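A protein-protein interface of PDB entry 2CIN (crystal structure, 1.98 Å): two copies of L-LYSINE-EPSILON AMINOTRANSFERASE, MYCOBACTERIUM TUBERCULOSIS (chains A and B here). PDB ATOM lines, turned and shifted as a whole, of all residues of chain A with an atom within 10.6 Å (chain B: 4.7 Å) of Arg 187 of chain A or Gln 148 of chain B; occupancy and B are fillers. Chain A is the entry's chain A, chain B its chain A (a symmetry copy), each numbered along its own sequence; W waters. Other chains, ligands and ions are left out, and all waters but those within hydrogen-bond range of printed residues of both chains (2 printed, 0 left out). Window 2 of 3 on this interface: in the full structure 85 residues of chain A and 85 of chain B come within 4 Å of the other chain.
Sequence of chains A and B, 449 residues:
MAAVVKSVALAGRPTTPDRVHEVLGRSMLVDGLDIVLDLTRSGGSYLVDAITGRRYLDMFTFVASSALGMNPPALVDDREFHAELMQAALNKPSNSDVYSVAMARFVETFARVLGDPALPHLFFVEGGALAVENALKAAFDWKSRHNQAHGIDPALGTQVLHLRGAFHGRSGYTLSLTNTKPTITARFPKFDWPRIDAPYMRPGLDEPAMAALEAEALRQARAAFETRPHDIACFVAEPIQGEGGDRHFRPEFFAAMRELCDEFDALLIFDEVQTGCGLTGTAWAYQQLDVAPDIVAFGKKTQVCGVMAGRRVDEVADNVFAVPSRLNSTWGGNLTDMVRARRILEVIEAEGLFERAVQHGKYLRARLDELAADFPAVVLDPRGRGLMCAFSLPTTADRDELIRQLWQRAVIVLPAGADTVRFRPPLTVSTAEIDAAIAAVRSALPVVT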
ATOM      1  N   LEU A 175      12.906  18.984 -25.106  1.00  0.00           N
ATOM      2  CA  LEU A 175      13.743  19.117 -23.903  1.00  0.00           C
ATOM      3  C   LEU A 175      14.921  20.055 -24.106  1.00  0.00           C
ATOM      4  O   LEU A 175      15.472  20.568 -23.141  1.00  0.00           O
ATOM      5  CB  LEU A 175      14.274  17.751 -23.463  1.00  0.00           C
ATOM      6  CG  LEU A 175      13.676  16.882 -22.330  1.00  0.00           C
ATOM      7  CD1 LEU A 175      12.553  17.432 -21.434  1.00  0.00           C
ATOM      8  CD2 LEU A 175      13.474  15.434 -22.771  1.00  0.00           C
ATOM      9  N   SER A 176      15.311  20.277 -25.359  1.00  0.00           N
ATOM     10  CA  SER A 176      16.370  21.247 -25.665  1.00  0.00           C
ATOM     11  C   SER A 176      15.834  22.666 -25.737  1.00  0.00           C
ATOM     12  O   SER A 176      16.596  23.624 -25.869  1.00  0.00           O
ATOM     13  CB  SER A 176      17.089  20.866 -26.960  1.00  0.00           C
ATOM     14  OG  SER A 176      17.796  19.632 -26.800  1.00  0.00           O
ATOM     15  N   LYS A 181      11.207  24.834 -15.052  1.00  0.00           N
ATOM     16  CA  LYS A 181      11.721  24.221 -13.829  1.00  0.00           C
ATOM     17  C   LYS A 181      12.806  23.198 -14.188  1.00  0.00           C
ATOM     18  O   LYS A 181      12.617  22.381 -15.099  1.00  0.00           O
ATOM     19  CB  LYS A 181      10.593  23.535 -13.005  1.00  0.00           C
ATOM     20  CG  LYS A 181       9.322  24.391 -12.670  1.00  0.00           C
ATOM     21  CD  LYS A 181       9.634  25.954 -12.614  1.00  0.00           C
ATOM     22  CE  LYS A 181       8.395  26.948 -12.774  1.00  0.00           C
ATOM     23  NZ  LYS A 181       7.466  26.852 -14.012  1.00  0.00           N
ATOM     24  N   PRO A 182      13.947  23.224 -13.468  1.00  0.00           N
ATOM     25  CA  PRO A 182      15.086  22.314 -13.691  1.00  0.00           C
ATOM     26  C   PRO A 182      14.692  20.840 -13.657  1.00  0.00           C
ATOM     27  O   PRO A 182      15.264  20.044 -14.381  1.00  0.00           O
ATOM     28  CB  PRO A 182      16.015  22.627 -12.503  1.00  0.00           C
ATOM     29  CG  PRO A 182      15.709  24.011 -12.154  1.00  0.00           C
ATOM     30  CD  PRO A 182      14.206  24.143 -12.348  1.00  0.00           C
ATOM     31  N   THR A 183      13.716  20.497 -12.811  1.00  0.00           N
ATOM     32  CA  THR A 183      13.145  19.148 -12.715  1.00  0.00           C
ATOM     33  C   THR A 183      12.755  18.558 -14.089  1.00  0.00           C
ATOM     34  O   THR A 183      12.883  17.362 -14.328  1.00  0.00           O
ATOM     35  CB  THR A 183      11.892  19.198 -11.787  1.00  0.00           C
ATOM     36  OG1 THR A 183      12.340  19.545 -10.478  1.00  0.00           O
ATOM     37  CG2 THR A 183      11.166  17.866 -11.706  1.00  0.00           C
ATOM     38  N   ILE A 184      12.278  19.403 -14.993  1.00  0.00           N
ATOM     39  CA  ILE A 184      11.811  18.905 -16.289  1.00  0.00           C
ATOM     40  C   ILE A 184      12.934  18.419 -17.191  1.00  0.00           C
ATOM     41  O   ILE A 184      12.752  17.459 -17.940  1.00  0.00           O
ATOM     42  CB  ILE A 184      10.928  19.959 -17.001  1.00  0.00           C
ATOM     43  CG1 ILE A 184       9.739  20.302 -16.094  1.00  0.00           C
ATOM     44  CG2 ILE A 184      10.462  19.462 -18.381  1.00  0.00           C
ATOM     45  CD1 ILE A 184       8.917  21.535 -16.572  1.00  0.00           C
ATOM     46  N   THR A 185      14.093  19.076 -17.109  1.00  0.00           N
ATOM     47  CA  THR A 185      15.143  18.877 -18.088  1.00  0.00           C
ATOM     48  C   THR A 185      16.437  18.279 -17.528  1.00  0.00           C
ATOM     49  O   THR A 185      17.279  17.879 -18.292  1.00  0.00           O
ATOM     50  CB  THR A 185      15.497  20.209 -18.810  1.00  0.00           C
ATOM     51  OG1 THR A 185      15.638  21.225 -17.826  1.00  0.00           O
ATOM     52  CG2 THR A 185      14.380  20.594 -19.759  1.00  0.00           C
ATOM     53  N   ALA A 186      16.584  18.196 -16.203  1.00  0.00           N
ATOM     54  CA  ALA A 186      17.893  17.828 -15.628  1.00  0.00           C
ATOM     55  C   ALA A 186      18.291  16.402 -15.990  1.00  0.00           C
ATOM     56  O   ALA A 186      17.435  15.495 -16.034  1.00  0.00           O
ATOM     57  CB  ALA A 186      17.887  18.039 -14.101  1.00  0.00           C
ATOM     58  N   ARG A 187      19.577  16.206 -16.299  1.00  0.00           N
ATOM     59  CA  ARG A 187      20.140  14.878 -16.581  1.00  0.00           C
ATOM     60  C   ARG A 187      19.671  14.244 -17.910  1.00  0.00           C
ATOM     61  O   ARG A 187      19.943  13.059 -18.145  1.00  0.00           O
ATOM     62  CB  ARG A 187      19.926  13.883 -15.411  1.00  0.00           C
ATOM     63  CG  ARG A 187      20.324  14.440 -14.020  1.00  0.00           C
ATOM     64  CD  ARG A 187      20.135  13.422 -12.911  1.00  0.00           C
ATOM     65  NE  ARG A 187      20.343  14.036 -11.592  1.00  0.00           N
ATOM     66  CZ  ARG A 187      21.436  13.893 -10.831  1.00  0.00           C
ATOM     67  NH1 ARG A 187      22.467  13.130 -11.212  1.00  0.00           N
ATOM     68  NH2 ARG A 187      21.477  14.498  -9.653  1.00  0.00           N
ATOM     69  N   PHE A 188      18.984  15.023 -18.758  1.00  0.00           N
ATOM     70  CA  PHE A 188      18.543  14.560 -20.094  1.00  0.00           C
ATOM     71  C   PHE A 188      19.432  15.218 -21.172  1.00  0.00           C
ATOM     72  O   PHE A 188      19.657  16.428 -21.112  1.00  0.00           O
ATOM     73  CB  PHE A 188      17.042  14.886 -20.289  1.00  0.00           C
ATOM     74  CG  PHE A 188      16.141  14.249 -19.231  1.00  0.00           C
ATOM     75  CD1 PHE A 188      16.335  12.906 -18.849  1.00  0.00           C
ATOM     76  CD2 PHE A 188      15.134  14.979 -18.606  1.00  0.00           C
ATOM     77  CE1 PHE A 188      15.539  12.304 -17.862  1.00  0.00           C
ATOM     78  CE2 PHE A 188      14.322  14.379 -17.615  1.00  0.00           C
ATOM     79  CZ  PHE A 188      14.518  13.034 -17.258  1.00  0.00           C
ATOM     80  N   PRO A 189      20.011  14.426 -22.095  1.00  0.00           N
ATOM     81  CA  PRO A 189      20.850  15.039 -23.122  1.00  0.00           C
ATOM     82  C   PRO A 189      20.122  16.080 -24.001  1.00  0.00           C
ATOM     83  O   PRO A 189      18.944  15.927 -24.344  1.00  0.00           O
ATOM     84  CB  PRO A 189      21.362  13.851 -23.959  1.00  0.00           C
ATOM     85  CG  PRO A 189      20.531  12.659 -23.544  1.00  0.00           C
ATOM     86  CD  PRO A 189      19.999  12.953 -22.181  1.00  0.00           C
ATOM     87  N   LYS A 190      20.855  17.122 -24.363  1.00  0.00           N
ATOM     88  CA  LYS A 190      20.258  18.266 -25.046  1.00  0.00           C
ATOM     89  C   LYS A 190      21.164  18.723 -26.192  1.00  0.00           C
ATOM     90  O   LYS A 190      22.368  18.504 -26.160  1.00  0.00           O
ATOM     91  CB  LYS A 190      20.013  19.405 -24.050  1.00  0.00           C
ATOM     92  CG  LYS A 190      18.903  19.111 -23.038  1.00  0.00           C
ATOM     93  CD  LYS A 190      18.679  20.234 -21.993  1.00  0.00           C
ATOM     94  CE  LYS A 190      19.624  20.150 -20.785  1.00  0.00           C
ATOM     95  NZ  LYS A 190      19.485  18.910 -19.924  1.00  0.00           N
ATOM     96  N   PHE B 140      18.839   7.543 -18.643  1.00  0.00           N
ATOM     97  CA  PHE B 140      19.779   8.667 -18.575  1.00  0.00           C
ATOM     98  C   PHE B 140      19.841   9.181 -17.126  1.00  0.00           C
ATOM     99  O   PHE B 140      20.925   9.425 -16.581  1.00  0.00           O
ATOM    100  CB  PHE B 140      19.338   9.842 -19.455  1.00  0.00           C
ATOM    101  CG  PHE B 140      19.304   9.544 -20.942  1.00  0.00           C
ATOM    102  CD1 PHE B 140      20.363   8.884 -21.575  1.00  0.00           C
ATOM    103  CD2 PHE B 140      18.244  10.023 -21.728  1.00  0.00           C
ATOM    104  CE1 PHE B 140      20.331   8.648 -22.962  1.00  0.00           C
ATOM    105  CE2 PHE B 140      18.216   9.785 -23.126  1.00  0.00           C
ATOM    106  CZ  PHE B 140      19.255   9.084 -23.731  1.00  0.00           C
ATOM    107  N   ASP B 141      18.669   9.338 -16.511  1.00  0.00           N
ATOM    108  CA  ASP B 141      18.568   9.749 -15.118  1.00  0.00           C
ATOM    109  C   ASP B 141      19.252   8.735 -14.174  1.00  0.00           C
ATOM    110  O   ASP B 141      20.001   9.121 -13.269  1.00  0.00           O
ATOM    111  CB  ASP B 141      17.097   9.914 -14.748  1.00  0.00           C
ATOM    112  CG  ASP B 141      16.895  10.203 -13.251  1.00  0.00           C
ATOM    113  OD1 ASP B 141      16.975  11.380 -12.846  1.00  0.00           O
ATOM    114  OD2 ASP B 141      16.640   9.242 -12.501  1.00  0.00           O
ATOM    115  N   SER B 144      23.194   8.790 -14.603  1.00  0.00           N
ATOM    116  CA  SER B 144      23.754  10.005 -14.037  1.00  0.00           C
ATOM    117  C   SER B 144      23.754   9.903 -12.501  1.00  0.00           C
ATOM    118  O   SER B 144      24.775  10.177 -11.872  1.00  0.00           O
ATOM    119  CB  SER B 144      22.954  11.228 -14.541  1.00  0.00           C
ATOM    120  OG  SER B 144      23.265  12.420 -13.845  1.00  0.00           O
ATOM    121  N   ARG B 145      22.626   9.477 -11.915  1.00  0.00           N
ATOM    122  CA  ARG B 145      22.497   9.332 -10.452  1.00  0.00           C
ATOM    123  C   ARG B 145      23.369   8.193  -9.887  1.00  0.00           C
ATOM    124  O   ARG B 145      23.963   8.356  -8.805  1.00  0.00           O
ATOM    125  CB  ARG B 145      21.032   9.203 -10.008  1.00  0.00           C
ATOM    126  CG  ARG B 145      20.198  10.357 -10.545  1.00  0.00           C
ATOM    127  CD  ARG B 145      18.696  10.317 -10.199  1.00  0.00           C
ATOM    128  NE  ARG B 145      18.578  11.268  -9.154  1.00  0.00           N
ATOM    129  CZ  ARG B 145      17.865  12.373  -9.115  1.00  0.00           C
ATOM    130  NH1 ARG B 145      17.000  12.724 -10.039  1.00  0.00           N
ATOM    131  NH2 ARG B 145      18.009  13.088  -8.032  1.00  0.00           N
ATOM    132  N   HIS B 146      23.479   7.091 -10.630  1.00  0.00           N
ATOM    133  CA  HIS B 146      24.361   5.968 -10.273  1.00  0.00           C
ATOM    134  C   HIS B 146      25.838   6.421 -10.303  1.00  0.00           C
ATOM    135  O   HIS B 146      26.594   6.201  -9.325  1.00  0.00           O
ATOM    136  CB  HIS B 146      24.123   4.760 -11.201  1.00  0.00           C
ATOM    137  CG  HIS B 146      24.837   3.505 -10.781  1.00  0.00           C
ATOM    138  ND1 HIS B 146      26.113   3.193 -11.202  1.00  0.00           N
ATOM    139  CD2 HIS B 146      24.434   2.469 -10.007  1.00  0.00           C
ATOM    140  CE1 HIS B 146      26.474   2.031 -10.688  1.00  0.00           C
ATOM    141  NE2 HIS B 146      25.474   1.573  -9.955  1.00  0.00           N
ATOM    142  N   ASN B 147      26.235   7.052 -11.410  1.00  0.00           N
ATOM    143  CA  ASN B 147      27.536   7.715 -11.528  1.00  0.00           C
ATOM    144  C   ASN B 147      27.822   8.602 -10.307  1.00  0.00           C
ATOM    145  O   ASN B 147      28.843   8.421  -9.629  1.00  0.00           O
ATOM    146  CB  ASN B 147      27.625   8.552 -12.810  1.00  0.00           C
ATOM    147  CG  ASN B 147      27.954   7.723 -14.041  1.00  0.00           C
ATOM    148  OD1 ASN B 147      28.307   6.538 -13.949  1.00  0.00           O
ATOM    149  ND2 ASN B 147      27.849   8.354 -15.214  1.00  0.00           N
ATOM    150  N   GLN B 148      26.914   9.531 -10.018  1.00  0.00           N
ATOM    151  CA  GLN B 148      27.069  10.454  -8.893  1.00  0.00           C
ATOM    152  C   GLN B 148      27.294   9.727  -7.562  1.00  0.00           C
ATOM    153  O   GLN B 148      28.146  10.143  -6.775  1.00  0.00           O
ATOM    154  CB  GLN B 148      25.845  11.358  -8.775  1.00  0.00           C
ATOM    155  CG  GLN B 148      26.043  12.577  -7.909  1.00  0.00           C
ATOM    156  CD  GLN B 148      24.829  13.498  -7.897  1.00  0.00           C
ATOM    157  OE1 GLN B 148      24.099  13.611  -8.878  1.00  0.00           O
ATOM    158  NE2 GLN B 148      24.609  14.155  -6.769  1.00  0.00           N
ATOM    159  N   ALA B 149      26.528   8.658  -7.322  1.00  0.00           N
ATOM    160  CA  ALA B 149      26.575   7.909  -6.071  1.00  0.00           C
ATOM    161  C   ALA B 149      27.887   7.141  -5.908  1.00  0.00           C
ATOM    162  O   ALA B 149      28.211   6.695  -4.804  1.00  0.00           O
ATOM    163  CB  ALA B 149      25.381   6.956  -5.973  1.00  0.00           C
ATOM    164  N   HIS B 150      28.618   6.973  -7.012  1.00  0.00           N
ATOM    165  CA  HIS B 150      29.893   6.266  -7.015  1.00  0.00           C
ATOM    166  C   HIS B 150      31.079   7.184  -7.364  1.00  0.00           C
ATOM    167  O   HIS B 150      32.085   6.729  -7.865  1.00  0.00           O
ATOM    168  CB  HIS B 150      29.832   5.037  -7.950  1.00  0.00           C
ATOM    169  CG  HIS B 150      28.766   4.051  -7.577  1.00  0.00           C
ATOM    170  ND1 HIS B 150      29.021   2.921  -6.830  1.00  0.00           N
ATOM    171  CD2 HIS B 150      27.433   4.044  -7.817  1.00  0.00           C
ATOM    172  CE1 HIS B 150      27.899   2.247  -6.646  1.00  0.00           C
ATOM    173  NE2 HIS B 150      26.916   2.915  -7.226  1.00  0.00           N
ATOM    174  N   GLY B 151      30.950   8.475  -7.101  1.00  0.00           N
ATOM    175  CA  GLY B 151      32.051   9.408  -7.305  1.00  0.00           C
ATOM    176  C   GLY B 151      32.414   9.713  -8.743  1.00  0.00           C
ATOM    177  O   GLY B 151      33.448  10.342  -9.002  1.00  0.00           O
ATOM    178  N   ILE B 152      31.576   9.272  -9.688  1.00  0.00           N
ATOM    179  CA  ILE B 152      31.716   9.631 -11.101  1.00  0.00           C
ATOM    180  C   ILE B 152      30.907  10.898 -11.439  1.00  0.00           C
ATOM    181  O   ILE B 152      29.832  11.138 -10.879  1.00  0.00           O
ATOM    182  CB  ILE B 152      31.332   8.431 -11.990  1.00  0.00           C
ATOM    183  CG1 ILE B 152      32.223   7.226 -11.639  1.00  0.00           C
ATOM    184  CG2 ILE B 152      31.455   8.776 -13.461  1.00  0.00           C
ATOM    185  CD1 ILE B 152      31.616   5.855 -11.951  1.00  0.00           C
ATOM    186  N   PRO B 154      28.333  13.343 -12.646  1.00  0.00           N
ATOM    187  CA  PRO B 154      26.926  13.149 -13.045  1.00  0.00           C
ATOM    188  C   PRO B 154      26.559  13.715 -14.427  1.00  0.00           C
ATOM    189  O   PRO B 154      25.440  13.499 -14.902  1.00  0.00           O
ATOM    190  CB  PRO B 154      26.143  13.860 -11.940  1.00  0.00           C
ATOM    191  CG  PRO B 154      27.086  14.895 -11.401  1.00  0.00           C
ATOM    192  CD  PRO B 154      28.439  14.239 -11.471  1.00  0.00           C
ATOM    193  N   ARG B 326       9.349  14.201 -13.095  1.00  0.00           N
ATOM    194  CA  ARG B 326      10.503  13.901 -13.959  1.00  0.00           C
ATOM    195  C   ARG B 326      10.034  13.392 -15.322  1.00  0.00           C
ATOM    196  O   ARG B 326      10.636  13.723 -16.339  1.00  0.00           O
ATOM    197  CB  ARG B 326      11.459  12.876 -13.316  1.00  0.00           C
ATOM    198  CG  ARG B 326      12.127  13.387 -12.034  1.00  0.00           C
ATOM    199  CD  ARG B 326      13.209  14.397 -12.325  1.00  0.00           C
ATOM    200  NE  ARG B 326      14.379  13.765 -12.919  1.00  0.00           N
ATOM    201  CZ  ARG B 326      15.142  14.311 -13.870  1.00  0.00           C
ATOM    202  NH1 ARG B 326      14.863  15.515 -14.371  1.00  0.00           N
ATOM    203  NH2 ARG B 326      16.199  13.650 -14.323  1.00  0.00           N
HETATM  204  O   HOH W   1      10.844  15.556 -18.329  1.00  0.00           O
HETATM  205  O   HOH W   2      22.432  11.710 -18.090  1.00  0.00           O
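Water W1 bridges O of Arg 326 of chain B and O of Ile 184 of chain A. Water W2 lies within hydrogen-bond range of the backbone carbonyl oxygen (O) of Arg 187 of chain A (2.8 Å) and the backbone carbonyl oxygen (O) of Phe 140 of chain B (3.1 Å).
NH1 of Arg 187 of chain A is in hydrogen-bond range of OG of Ser 144 of chain B, at 2.8 Å. The side-chain amide oxygen of Gln 148 of chain B lies within hydrogen-bond range of the guanidinium group of Arg 187 of chain A (2.9 Å). The backbone carbonyl oxygen (O) of Ala 186 of chain A lies within hydrogen-bond range of the guanidinium group (NH2) of Arg 326 of chain B (2.8 Å). O of Thr 183 of chain A lies within hydrogen-bond range of NH1 of Arg 326 of chain B (2.7 Å).
No position is printed for both chains. Of the 11 pairs that touch across the chains among the printed residues, none has its exchanged pair printed and touching as well.
Of the 13 printed residues of chain B, 7 touch a printed residue of chain A. Printed residues of chain A that touch a printed residue of chain B: Thr 183, Ala 186, Arg 187, Phe 188 and Pro 189. Hydrophobic or aromatic side chains of chain A that line the printed part of chain B: Ala 186, Phe 188 and Pro 189. Among the printed residues, 11 pairs touch across the chains. Among the printed residues, no Asp or Glu carboxylate lies within 4 Å of a Lys or Arg side-chain nitrogen of the other chain.
Among the printed residues, pairs that only touch across the chains: Arg 187 of chain A with Phe 140 of chain B (3.5 Å), Arg 187 of chain A with Asp 141 of chain B (3.8 Å), Arg 187 of chain A with Arg 145 of chain B (3.6 Å), Arg 187 of chain A with Pro 154 of chain B (3.8 Å), Arg 187 of chain A with Arg 326 of chain B (3.9 Å), Phe 188 of chain A with Arg 326 of chain B (3.4 Å) and Pro 189 of chain A with Phe 140 of chain B (3.4 Å).
Of the printed residues of chain B, Thr 183 of chain A touches Arg 326 (2.7 Å). Of chain B, only Phe 140 (3.5 Å), Asp 141 (3.8 Å), Ser 144 (2.8 Å), Arg 145 (3.6 Å), Gln 148 (2.9 Å), Pro 154 (3.8 Å) and Arg 326 (3.9 Å) come within 4 Å of Arg 187 of chain A. Of the printed residues of chain B, Phe 188 of chain A touches Arg 326 (3.4 Å). Printed residues of chain A within 4 Å of Phe 140 of chain B: Arg 187 and Pro 189. Printed residues of chain A within 4 Å of Asp 141 of chain B: Arg 187 (3.8 Å). No residue of chain A comes within 4 Å of Asn 147 of chain B. Gln 148 of chain B touches just one residue of chain A: Arg 187 (2.9 Å). No residue of chain A comes within 4 Å of Ala 149 of chain B. Gly 151 of chain B touches none of the printed residues of chain A. Of chain A, only Arg 187 comes within 4 Å of Pro 154 of chain B. The nearest printed residue of chain B that does not touch Arg 187 of chain A is His 146 of chain B (6.2 Å). The nearest residue of chain A that does not touch Gln 148 of chain B is Ala 186 of chain A (9.2 Å).
The side-chain carboxylate (OD1) of Asp 141 of chain B is in salt-bridge range of the guanidinium group (NH2) of Arg 326 of chain B (2.8 Å). O of Phe 188 of chain A is in hydrogen-bond range of NZ of Lys 190 of chain A (2.8 Å). The guanidinium group of Arg 145 of chain B lies within salt-bridge range of the side-chain carboxylate of Asp 141 of chain B, 3.1 Å away. OG of Ser 144 of chain B sits at hydrogen-bond distance from O of Pro 154 of chain B (2.6 Å).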
